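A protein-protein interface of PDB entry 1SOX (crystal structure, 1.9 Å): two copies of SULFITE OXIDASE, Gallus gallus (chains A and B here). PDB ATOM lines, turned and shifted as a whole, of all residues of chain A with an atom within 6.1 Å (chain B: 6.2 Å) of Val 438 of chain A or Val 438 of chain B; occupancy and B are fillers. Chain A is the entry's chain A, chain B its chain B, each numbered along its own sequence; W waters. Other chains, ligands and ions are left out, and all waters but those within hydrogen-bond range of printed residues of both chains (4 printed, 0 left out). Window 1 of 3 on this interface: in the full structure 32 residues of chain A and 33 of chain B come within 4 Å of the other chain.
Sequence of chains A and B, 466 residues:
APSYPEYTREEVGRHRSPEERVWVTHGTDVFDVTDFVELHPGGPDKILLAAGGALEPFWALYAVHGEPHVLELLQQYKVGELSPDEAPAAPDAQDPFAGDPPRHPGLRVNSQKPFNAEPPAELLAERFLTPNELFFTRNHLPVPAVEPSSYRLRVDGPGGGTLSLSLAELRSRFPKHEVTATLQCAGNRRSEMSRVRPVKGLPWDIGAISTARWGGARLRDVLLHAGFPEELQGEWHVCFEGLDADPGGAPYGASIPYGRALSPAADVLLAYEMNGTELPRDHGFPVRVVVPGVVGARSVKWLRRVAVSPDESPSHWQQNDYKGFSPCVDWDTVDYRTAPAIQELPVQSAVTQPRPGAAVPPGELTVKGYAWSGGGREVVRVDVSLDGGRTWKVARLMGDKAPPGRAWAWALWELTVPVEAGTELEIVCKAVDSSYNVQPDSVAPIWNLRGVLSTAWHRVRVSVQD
The backbone NH (N) of Val 347 of chain B is in hydrogen-bond range of the side-chain amide oxygen (OD1) of Asn 437 of chain A, at 3.4 Å.
ND2 of Asn 437 of chain A lies close to ND2 of Asn 437 of chain B.
N of Tyr 436 of chain A is in hydrogen-bond range of OD1 of Asp 433 of chain A, at 3.3 Å.
The backbone NH of Asn 437 of chain A sits at hydrogen-bond distance from the side-chain carboxylate of Asp 433 of chain A (3.0 Å).
The backbone NH (N) of Ala 431 of chain B is in hydrogen-bond range of the side-chain amide oxygen (OE1) of Gln 439 of chain B (2.8 Å).
The backbone NH (N) of Tyr 436 of chain B lies within hydrogen-bond range of the side-chain carboxylate (OD1) of Asp 433 of chain B (3.2 Å).
OD1 of Asp 433 of chain B is in hydrogen-bond range of N of Asn 437 of chain B.
NE2 of Gln 439 of chain B lies within hydrogen-bond range of O of Thr 455 of chain B (2.9 Å).
Among the printed residues, pairs that only touch across the chains: Pro 346 of chain A with Tyr 436 of chain B (3.4 Å), Pro 346 of chain A with Asn 437 of chain B (3.6 Å), Tyr 436 of chain A with Pro 346 of chain B (3.2 Å), Asn 437 of chain A with Pro 346 of chain B (3.3 Å), Val 438 of chain A with Val 438 of chain B (3.9 Å), Val 438 of chain A with Pro 440 of chain B (3.9 Å), Pro 440 of chain A with Val 438 of chain B (3.6 Å), Pro 440 of chain A with Gln 439 of chain B (3.9 Å) and Pro 440 of chain A with Pro 440 of chain B (3.9 Å).
Val 438 of chain A touches just these residues of chain B: Val 438 (3.9 Å) and Pro 440 (3.9 Å).
Val 438 of chain B touches just these residues of chain A: Val 438 and Pro 440.
Of the printed residues of chain B, Tyr 436 of chain A touches Pro 346.
Of the printed residues of chain A, Val 347 of chain B touches Asn 437.
Val 432 of chain B touches none of the printed residues of chain A.
Printed residues of chain A that touch a printed residue of chain B: Pro 346, Tyr 436, Asn 437, Val 438 and Pro 440.
Hydrophobic or aromatic side chains of chain A within 4 Å of the printed part of chain B: Pro 346, Val 438 and Pro 440.
Of the 12 printed residues of chain B, 7 touch a printed residue of chain A.
Among the printed residues, 11 pairs touch across the chains.
Among the printed residues, no Asp or Glu carboxylate lies within 4 Å of a Lys or Arg side-chain nitrogen of the other chain.
Pro 346 of chain A touches Tyr 436 of chain B, and with the chains exchanged Tyr 436 of chain A touches Pro 346 of chain B.
Asn 437 of chain A touches Val 347 of chain B, but with the chains exchanged Val 347 of chain A does not touch Asn 437 of chain B (4.02 Å).
Val 438 of chain A touches Pro 440 of chain B, and with the chains exchanged Pro 440 of chain A touches Val 438 of chain B.
Pro 440 of chain A touches Gln 439 of chain B, but with the chains exchanged Gln 439 of chain A does not touch Pro 440 of chain B (4.2 Å).
12 positions are printed for both chains.
Of the 11 pairs that touch across the chains among the printed residues, 9 have their exchanged pair printed and touching as well.
Water W3 lies within hydrogen-bond range of the side-chain amide oxygen of Asn 437 of chain B (2.5 Å), the side-chain carboxylate of Asp 433 of chain A (2.7 Å) and the backbone NH of Val 347 of chain A (3.1 Å).
Water W4 lies within hydrogen-bond range of the side-chain amide oxygen (OD1) of Asn 437 of chain A (2.6 Å), the backbone carbonyl oxygen (O) of Val 438 of chain B (2.8 Å) and the backbone NH (N) of Val 438 of chain A (3.1 Å).
Water W2 bridges the backbone carbonyl oxygen of Val 438 of chain B (2.8 Å) and the backbone carbonyl oxygen of Val 438 of chain A (2.9 Å).
Water W1 lies within hydrogen-bond range of O of Val 438 of chain A (2.8 Å), OD1 of Asn 437 of chain B (3.0 Å) and N of Val 438 of chain B (3.1 Å).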
ATOM      1  N   PRO A 346      20.951  25.694 -12.450  1.00  0.00           N
ATOM      2  CA  PRO A 346      20.809  24.517 -11.588  1.00  0.00           C
ATOM      3  C   PRO A 346      20.815  23.214 -12.358  1.00  0.00           C
ATOM      4  O   PRO A 346      20.678  23.214 -13.579  1.00  0.00           O
ATOM      5  CB  PRO A 346      19.482  24.723 -10.838  1.00  0.00           C
ATOM      6  CG  PRO A 346      18.698  25.490 -11.886  1.00  0.00           C
ATOM      7  CD  PRO A 346      19.672  26.354 -12.668  1.00  0.00           C
ATOM      8  N   VAL A 347      20.905  22.087 -11.641  1.00  0.00           N
ATOM      9  CA  VAL A 347      20.990  20.772 -12.285  1.00  0.00           C
ATOM     10  C   VAL A 347      19.733  20.510 -13.112  1.00  0.00           C
ATOM     11  O   VAL A 347      18.670  20.902 -12.672  1.00  0.00           O
ATOM     12  CB  VAL A 347      21.222  19.665 -11.253  1.00  0.00           C
ATOM     13  CG1 VAL A 347      20.156  19.709 -10.170  1.00  0.00           C
ATOM     14  CG2 VAL A 347      21.365  18.291 -11.893  1.00  0.00           C
ATOM     15  N   LYS A 430      15.818  12.127 -13.278  1.00  0.00           N
ATOM     16  CA  LYS A 430      16.235  13.224 -12.394  1.00  0.00           C
ATOM     17  C   LYS A 430      17.743  13.068 -12.197  1.00  0.00           C
ATOM     18  O   LYS A 430      18.241  11.934 -12.185  1.00  0.00           O
ATOM     19  CB  LYS A 430      15.488  13.280 -11.083  1.00  0.00           C
ATOM     20  CG  LYS A 430      15.702  12.024 -10.208  1.00  0.00           C
ATOM     21  CD  LYS A 430      14.800  12.146  -8.979  1.00  0.00           C
ATOM     22  CE  LYS A 430      14.909  10.863  -8.117  1.00  0.00           C
ATOM     23  NZ  LYS A 430      16.209  10.919  -7.369  1.00  0.00           N
ATOM     24  N   ALA A 431      18.473  14.183 -12.167  1.00  0.00           N
ATOM     25  CA  ALA A 431      19.924  14.090 -12.038  1.00  0.00           C
ATOM     26  C   ALA A 431      20.437  14.720 -10.747  1.00  0.00           C
ATOM     27  O   ALA A 431      19.748  15.540 -10.133  1.00  0.00           O
ATOM     28  CB  ALA A 431      20.579  14.808 -13.213  1.00  0.00           C
ATOM     29  N   VAL A 432      21.639  14.286 -10.376  1.00  0.00           N
ATOM     30  CA  VAL A 432      22.316  14.758  -9.163  1.00  0.00           C
ATOM     31  C   VAL A 432      23.699  15.280  -9.535  1.00  0.00           C
ATOM     32  O   VAL A 432      24.440  14.588 -10.283  1.00  0.00           O
ATOM     33  CB  VAL A 432      22.505  13.611  -8.138  1.00  0.00           C
ATOM     34  CG1 VAL A 432      23.123  14.156  -6.847  1.00  0.00           C
ATOM     35  CG2 VAL A 432      21.165  12.978  -7.779  1.00  0.00           C
ATOM     36  N   ASP A 433      24.081  16.477  -9.049  1.00  0.00           N
ATOM     37  CA  ASP A 433      25.384  16.992  -9.489  1.00  0.00           C
ATOM     38  C   ASP A 433      26.445  16.767  -8.420  1.00  0.00           C
ATOM     39  O   ASP A 433      26.229  16.196  -7.353  1.00  0.00           O
ATOM     40  CB  ASP A 433      25.281  18.445 -10.002  1.00  0.00           C
ATOM     41  CG  ASP A 433      25.104  19.499  -8.941  1.00  0.00           C
ATOM     42  OD1 ASP A 433      25.263  19.260  -7.742  1.00  0.00           O
ATOM     43  OD2 ASP A 433      24.851  20.700  -9.287  1.00  0.00           O
ATOM     44  N   TYR A 436      25.814  17.598  -4.947  1.00  0.00           N
ATOM     45  CA  TYR A 436      24.635  16.823  -4.566  1.00  0.00           C
ATOM     46  C   TYR A 436      23.350  17.656  -4.622  1.00  0.00           C
ATOM     47  O   TYR A 436      22.366  17.398  -3.918  1.00  0.00           O
ATOM     48  CB  TYR A 436      24.797  16.121  -3.218  1.00  0.00           C
ATOM     49  CG  TYR A 436      25.628  14.845  -3.324  1.00  0.00           C
ATOM     50  CD1 TYR A 436      25.001  13.643  -3.636  1.00  0.00           C
ATOM     51  CD2 TYR A 436      26.990  14.821  -3.084  1.00  0.00           C
ATOM     52  CE1 TYR A 436      25.716  12.468  -3.718  1.00  0.00           C
ATOM     53  CE2 TYR A 436      27.732  13.637  -3.171  1.00  0.00           C
ATOM     54  CZ  TYR A 436      27.084  12.469  -3.492  1.00  0.00           C
ATOM     55  OH  TYR A 436      27.778  11.267  -3.584  1.00  0.00           O
ATOM     56  N   ASN A 437      23.311  18.610  -5.562  1.00  0.00           N
ATOM     57  CA  ASN A 437      22.050  19.345  -5.775  1.00  0.00           C
ATOM     58  C   ASN A 437      21.196  18.412  -6.632  1.00  0.00           C
ATOM     59  O   ASN A 437      21.703  17.632  -7.465  1.00  0.00           O
ATOM     60  CB  ASN A 437      22.310  20.714  -6.406  1.00  0.00           C
ATOM     61  CG  ASN A 437      22.419  21.756  -5.311  1.00  0.00           C
ATOM     62  OD1 ASN A 437      21.481  22.058  -4.561  1.00  0.00           O
ATOM     63  ND2 ASN A 437      23.595  22.333  -5.097  1.00  0.00           N
ATOM     64  N   VAL A 438      19.890  18.467  -6.434  1.00  0.00           N
ATOM     65  CA  VAL A 438      18.926  17.597  -7.100  1.00  0.00           C
ATOM     66  C   VAL A 438      17.792  18.389  -7.751  1.00  0.00           C
ATOM     67  O   VAL A 438      17.679  19.584  -7.518  1.00  0.00           O
ATOM     68  CB  VAL A 438      18.316  16.610  -6.073  1.00  0.00           C
ATOM     69  CG1 VAL A 438      19.391  15.708  -5.455  1.00  0.00           C
ATOM     70  CG2 VAL A 438      17.622  17.385  -4.960  1.00  0.00           C
ATOM     71  N   GLN A 439      16.988  17.742  -8.571  1.00  0.00           N
ATOM     72  CA  GLN A 439      15.835  18.418  -9.220  1.00  0.00           C
ATOM     73  C   GLN A 439      14.571  18.175  -8.423  1.00  0.00           C
ATOM     74  O   GLN A 439      14.355  17.101  -7.865  1.00  0.00           O
ATOM     75  CB  GLN A 439      15.641  17.802 -10.595  1.00  0.00           C
ATOM     76  CG  GLN A 439      16.724  18.089 -11.604  1.00  0.00           C
ATOM     77  CD  GLN A 439      16.526  17.380 -12.903  1.00  0.00           C
ATOM     78  OE1 GLN A 439      17.246  16.440 -13.276  1.00  0.00           O
ATOM     79  NE2 GLN A 439      15.534  17.851 -13.677  1.00  0.00           N
ATOM     80  N   PRO A 440      13.672  19.156  -8.374  1.00  0.00           N
ATOM     81  CA  PRO A 440      12.439  19.069  -7.595  1.00  0.00           C
ATOM     82  C   PRO A 440      11.350  18.272  -8.305  1.00  0.00           C
ATOM     83  O   PRO A 440      11.338  18.164  -9.533  1.00  0.00           O
ATOM     84  CB  PRO A 440      12.036  20.534  -7.333  1.00  0.00           C
ATOM     85  CG  PRO A 440      12.509  21.160  -8.618  1.00  0.00           C
ATOM     86  CD  PRO A 440      13.822  20.455  -9.021  1.00  0.00           C
ATOM     87  N   ILE A 446       7.961  25.763  -8.418  1.00  0.00           N
ATOM     88  CA  ILE A 446       9.027  26.524  -9.054  1.00  0.00           C
ATOM     89  C   ILE A 446       8.501  27.400 -10.189  1.00  0.00           C
ATOM     90  O   ILE A 446       9.255  27.987 -10.986  1.00  0.00           O
ATOM     91  CB  ILE A 446      10.175  25.640  -9.608  1.00  0.00           C
ATOM     92  CG1 ILE A 446       9.676  24.675 -10.653  1.00  0.00           C
ATOM     93  CG2 ILE A 446      10.819  24.937  -8.406  1.00  0.00           C
ATOM     94  CD1 ILE A 446      10.677  24.098 -11.618  1.00  0.00           C
ATOM     95  N   THR A 455      13.244  23.125 -14.179  1.00  0.00           N
ATOM     96  CA  THR A 455      14.074  21.950 -13.933  1.00  0.00           C
ATOM     97  C   THR A 455      13.401  20.868 -13.091  1.00  0.00           C
ATOM     98  O   THR A 455      14.078  19.961 -12.612  1.00  0.00           O
ATOM     99  CB  THR A 455      15.373  22.358 -13.198  1.00  0.00           C
ATOM    100  OG1 THR A 455      15.028  22.794 -11.887  1.00  0.00           O
ATOM    101  CG2 THR A 455      16.151  23.456 -13.923  1.00  0.00           C
ATOM    102  N   PRO B 346      24.151  20.539  -0.783  1.00  0.00           N
ATOM    103  CA  PRO B 346      23.089  21.215  -1.547  1.00  0.00           C
ATOM    104  C   PRO B 346      22.316  22.191  -0.710  1.00  0.00           C
ATOM    105  O   PRO B 346      22.335  22.210   0.524  1.00  0.00           O
ATOM    106  CB  PRO B 346      22.212  20.053  -2.074  1.00  0.00           C
ATOM    107  CG  PRO B 346      22.345  19.078  -0.910  1.00  0.00           C
ATOM    108  CD  PRO B 346      23.789  19.180  -0.412  1.00  0.00           C
ATOM    109  N   VAL B 347      21.519  23.076  -1.368  1.00  0.00           N
ATOM    110  CA  VAL B 347      20.697  24.061  -0.644  1.00  0.00           C
ATOM    111  C   VAL B 347      19.783  23.429   0.381  1.00  0.00           C
ATOM    112  O   VAL B 347      19.191  22.358   0.214  1.00  0.00           O
ATOM    113  CB  VAL B 347      19.897  24.916  -1.678  1.00  0.00           C
ATOM    114  CG1 VAL B 347      18.969  24.034  -2.499  1.00  0.00           C
ATOM    115  CG2 VAL B 347      19.158  26.028  -0.931  1.00  0.00           C
ATOM    116  N   ALA B 431      14.286  27.018   0.138  1.00  0.00           N
ATOM    117  CA  ALA B 431      15.221  28.074  -0.228  1.00  0.00           C
ATOM    118  C   ALA B 431      15.777  27.905  -1.608  1.00  0.00           C
ATOM    119  O   ALA B 431      15.780  26.849  -2.271  1.00  0.00           O
ATOM    120  CB  ALA B 431      16.299  28.098   0.863  1.00  0.00           C
ATOM    121  N   VAL B 432      16.276  29.044  -2.130  1.00  0.00           N
ATOM    122  CA  VAL B 432      16.864  29.124  -3.460  1.00  0.00           C
ATOM    123  C   VAL B 432      18.265  29.746  -3.330  1.00  0.00           C
ATOM    124  O   VAL B 432      18.356  30.768  -2.613  1.00  0.00           O
ATOM    125  CB  VAL B 432      16.080  30.062  -4.404  1.00  0.00           C
ATOM    126  CG1 VAL B 432      16.754  30.096  -5.770  1.00  0.00           C
ATOM    127  CG2 VAL B 432      14.617  29.654  -4.531  1.00  0.00           C
ATOM    128  N   ASP B 433      19.247  29.162  -4.005  1.00  0.00           N
ATOM    129  CA  ASP B 433      20.598  29.713  -3.860  1.00  0.00           C
ATOM    130  C   ASP B 433      20.929  30.536  -5.100  1.00  0.00           C
ATOM    131  O   ASP B 433      20.119  30.741  -6.000  1.00  0.00           O
ATOM    132  CB  ASP B 433      21.671  28.708  -3.512  1.00  0.00           C
ATOM    133  CG  ASP B 433      22.161  27.789  -4.597  1.00  0.00           C
ATOM    134  OD1 ASP B 433      21.862  27.967  -5.777  1.00  0.00           O
ATOM    135  OD2 ASP B 433      22.908  26.828  -4.235  1.00  0.00           O
ATOM    136  N   TYR B 436      20.608  29.248  -8.447  1.00  0.00           N
ATOM    137  CA  TYR B 436      19.189  28.983  -8.498  1.00  0.00           C
ATOM    138  C   TYR B 436      18.891  27.495  -8.277  1.00  0.00           C
ATOM    139  O   TYR B 436      17.921  26.989  -8.821  1.00  0.00           O
ATOM    140  CB  TYR B 436      18.563  29.484  -9.807  1.00  0.00           C
ATOM    141  CG  TYR B 436      18.247  30.972  -9.776  1.00  0.00           C
ATOM    142  CD1 TYR B 436      17.083  31.436  -9.175  1.00  0.00           C
ATOM    143  CD2 TYR B 436      19.103  31.887 -10.353  1.00  0.00           C
ATOM    144  CE1 TYR B 436      16.768  32.786  -9.128  1.00  0.00           C
ATOM    145  CE2 TYR B 436      18.792  33.241 -10.332  1.00  0.00           C
ATOM    146  CZ  TYR B 436      17.643  33.678  -9.731  1.00  0.00           C
ATOM    147  OH  TYR B 436      17.358  35.035  -9.725  1.00  0.00           O
ATOM    148  N   ASN B 437      19.676  26.873  -7.386  1.00  0.00           N
ATOM    149  CA  ASN B 437      19.350  25.507  -6.992  1.00  0.00           C
ATOM    150  C   ASN B 437      18.127  25.634  -6.089  1.00  0.00           C
ATOM    151  O   ASN B 437      17.965  26.628  -5.364  1.00  0.00           O
ATOM    152  CB  ASN B 437      20.434  24.868  -6.115  1.00  0.00           C
ATOM    153  CG  ASN B 437      21.523  24.306  -7.007  1.00  0.00           C
ATOM    154  OD1 ASN B 437      21.193  23.561  -7.917  1.00  0.00           O
ATOM    155  ND2 ASN B 437      22.743  24.736  -6.654  1.00  0.00           N
ATOM    156  N   VAL B 438      17.326  24.579  -6.046  1.00  0.00           N
ATOM    157  CA  VAL B 438      16.127  24.556  -5.230  1.00  0.00           C
ATOM    158  C   VAL B 438      16.032  23.231  -4.468  1.00  0.00           C
ATOM    159  O   VAL B 438      16.755  22.295  -4.820  1.00  0.00           O
ATOM    160  CB  VAL B 438      14.850  24.692  -6.105  1.00  0.00           C
ATOM    161  CG1 VAL B 438      14.796  26.014  -6.874  1.00  0.00           C
ATOM    162  CG2 VAL B 438      14.716  23.527  -7.067  1.00  0.00           C
ATOM    163  N   GLN B 439      15.202  23.183  -3.456  1.00  0.00           N
ATOM    164  CA  GLN B 439      14.997  21.985  -2.642  1.00  0.00           C
ATOM    165  C   GLN B 439      13.793  21.202  -3.190  1.00  0.00           C
ATOM    166  O   GLN B 439      12.823  21.771  -3.727  1.00  0.00           O
ATOM    167  CB  GLN B 439      14.673  22.378  -1.206  1.00  0.00           C
ATOM    168  CG  GLN B 439      15.777  23.013  -0.385  1.00  0.00           C
ATOM    169  CD  GLN B 439      15.275  23.461   0.960  1.00  0.00           C
ATOM    170  OE1 GLN B 439      15.132  24.643   1.259  1.00  0.00           O
ATOM    171  NE2 GLN B 439      14.964  22.504   1.849  1.00  0.00           N
ATOM    172  N   PRO B 440      13.878  19.894  -3.124  1.00  0.00           N
ATOM    173  CA  PRO B 440      12.889  18.981  -3.693  1.00  0.00           C
ATOM    174  C   PRO B 440      11.661  18.871  -2.817  1.00  0.00           C
ATOM    175  O   PRO B 440      11.704  19.031  -1.594  1.00  0.00           O
ATOM    176  CB  PRO B 440      13.587  17.597  -3.783  1.00  0.00           C
ATOM    177  CG  PRO B 440      14.493  17.714  -2.564  1.00  0.00           C
ATOM    178  CD  PRO B 440      15.041  19.154  -2.580  1.00  0.00           C
ATOM    179  N   ILE B 446      14.543  11.182  -2.659  1.00  0.00           N
ATOM    180  CA  ILE B 446      15.952  11.431  -2.285  1.00  0.00           C
ATOM    181  C   ILE B 446      16.377  10.522  -1.132  1.00  0.00           C
ATOM    182  O   ILE B 446      17.422  10.720  -0.502  1.00  0.00           O
ATOM    183  CB  ILE B 446      16.180  12.893  -1.882  1.00  0.00           C
ATOM    184  CG1 ILE B 446      15.256  13.321  -0.744  1.00  0.00           C
ATOM    185  CG2 ILE B 446      15.968  13.808  -3.093  1.00  0.00           C
ATOM    186  CD1 ILE B 446      15.828  14.422   0.123  1.00  0.00           C
ATOM    187  N   THR B 455      17.237  17.147   2.344  1.00  0.00           N
ATOM    188  CA  THR B 455      16.925  18.524   2.057  1.00  0.00           C
ATOM    189  C   THR B 455      15.558  18.747   1.392  1.00  0.00           C
ATOM    190  O   THR B 455      15.330  19.824   0.836  1.00  0.00           O
ATOM    191  CB  THR B 455      17.939  19.152   1.064  1.00  0.00           C
ATOM    192  OG1 THR B 455      17.836  18.427  -0.169  1.00  0.00           O
ATOM    193  CG2 THR B 455      19.373  19.072   1.549  1.00  0.00           C
HETATM  194  O   HOH W   1      18.423  22.315  -7.793  1.00  0.00           O
HETATM  195  O   HOH W   2      15.345  20.115  -5.867  1.00  0.00           O
HETATM  196  O   HOH W   3      22.935  22.535  -9.409  1.00  0.00           O
HETATM  197  O   HOH W   4      19.147  20.808  -4.593  1.00  0.00           O
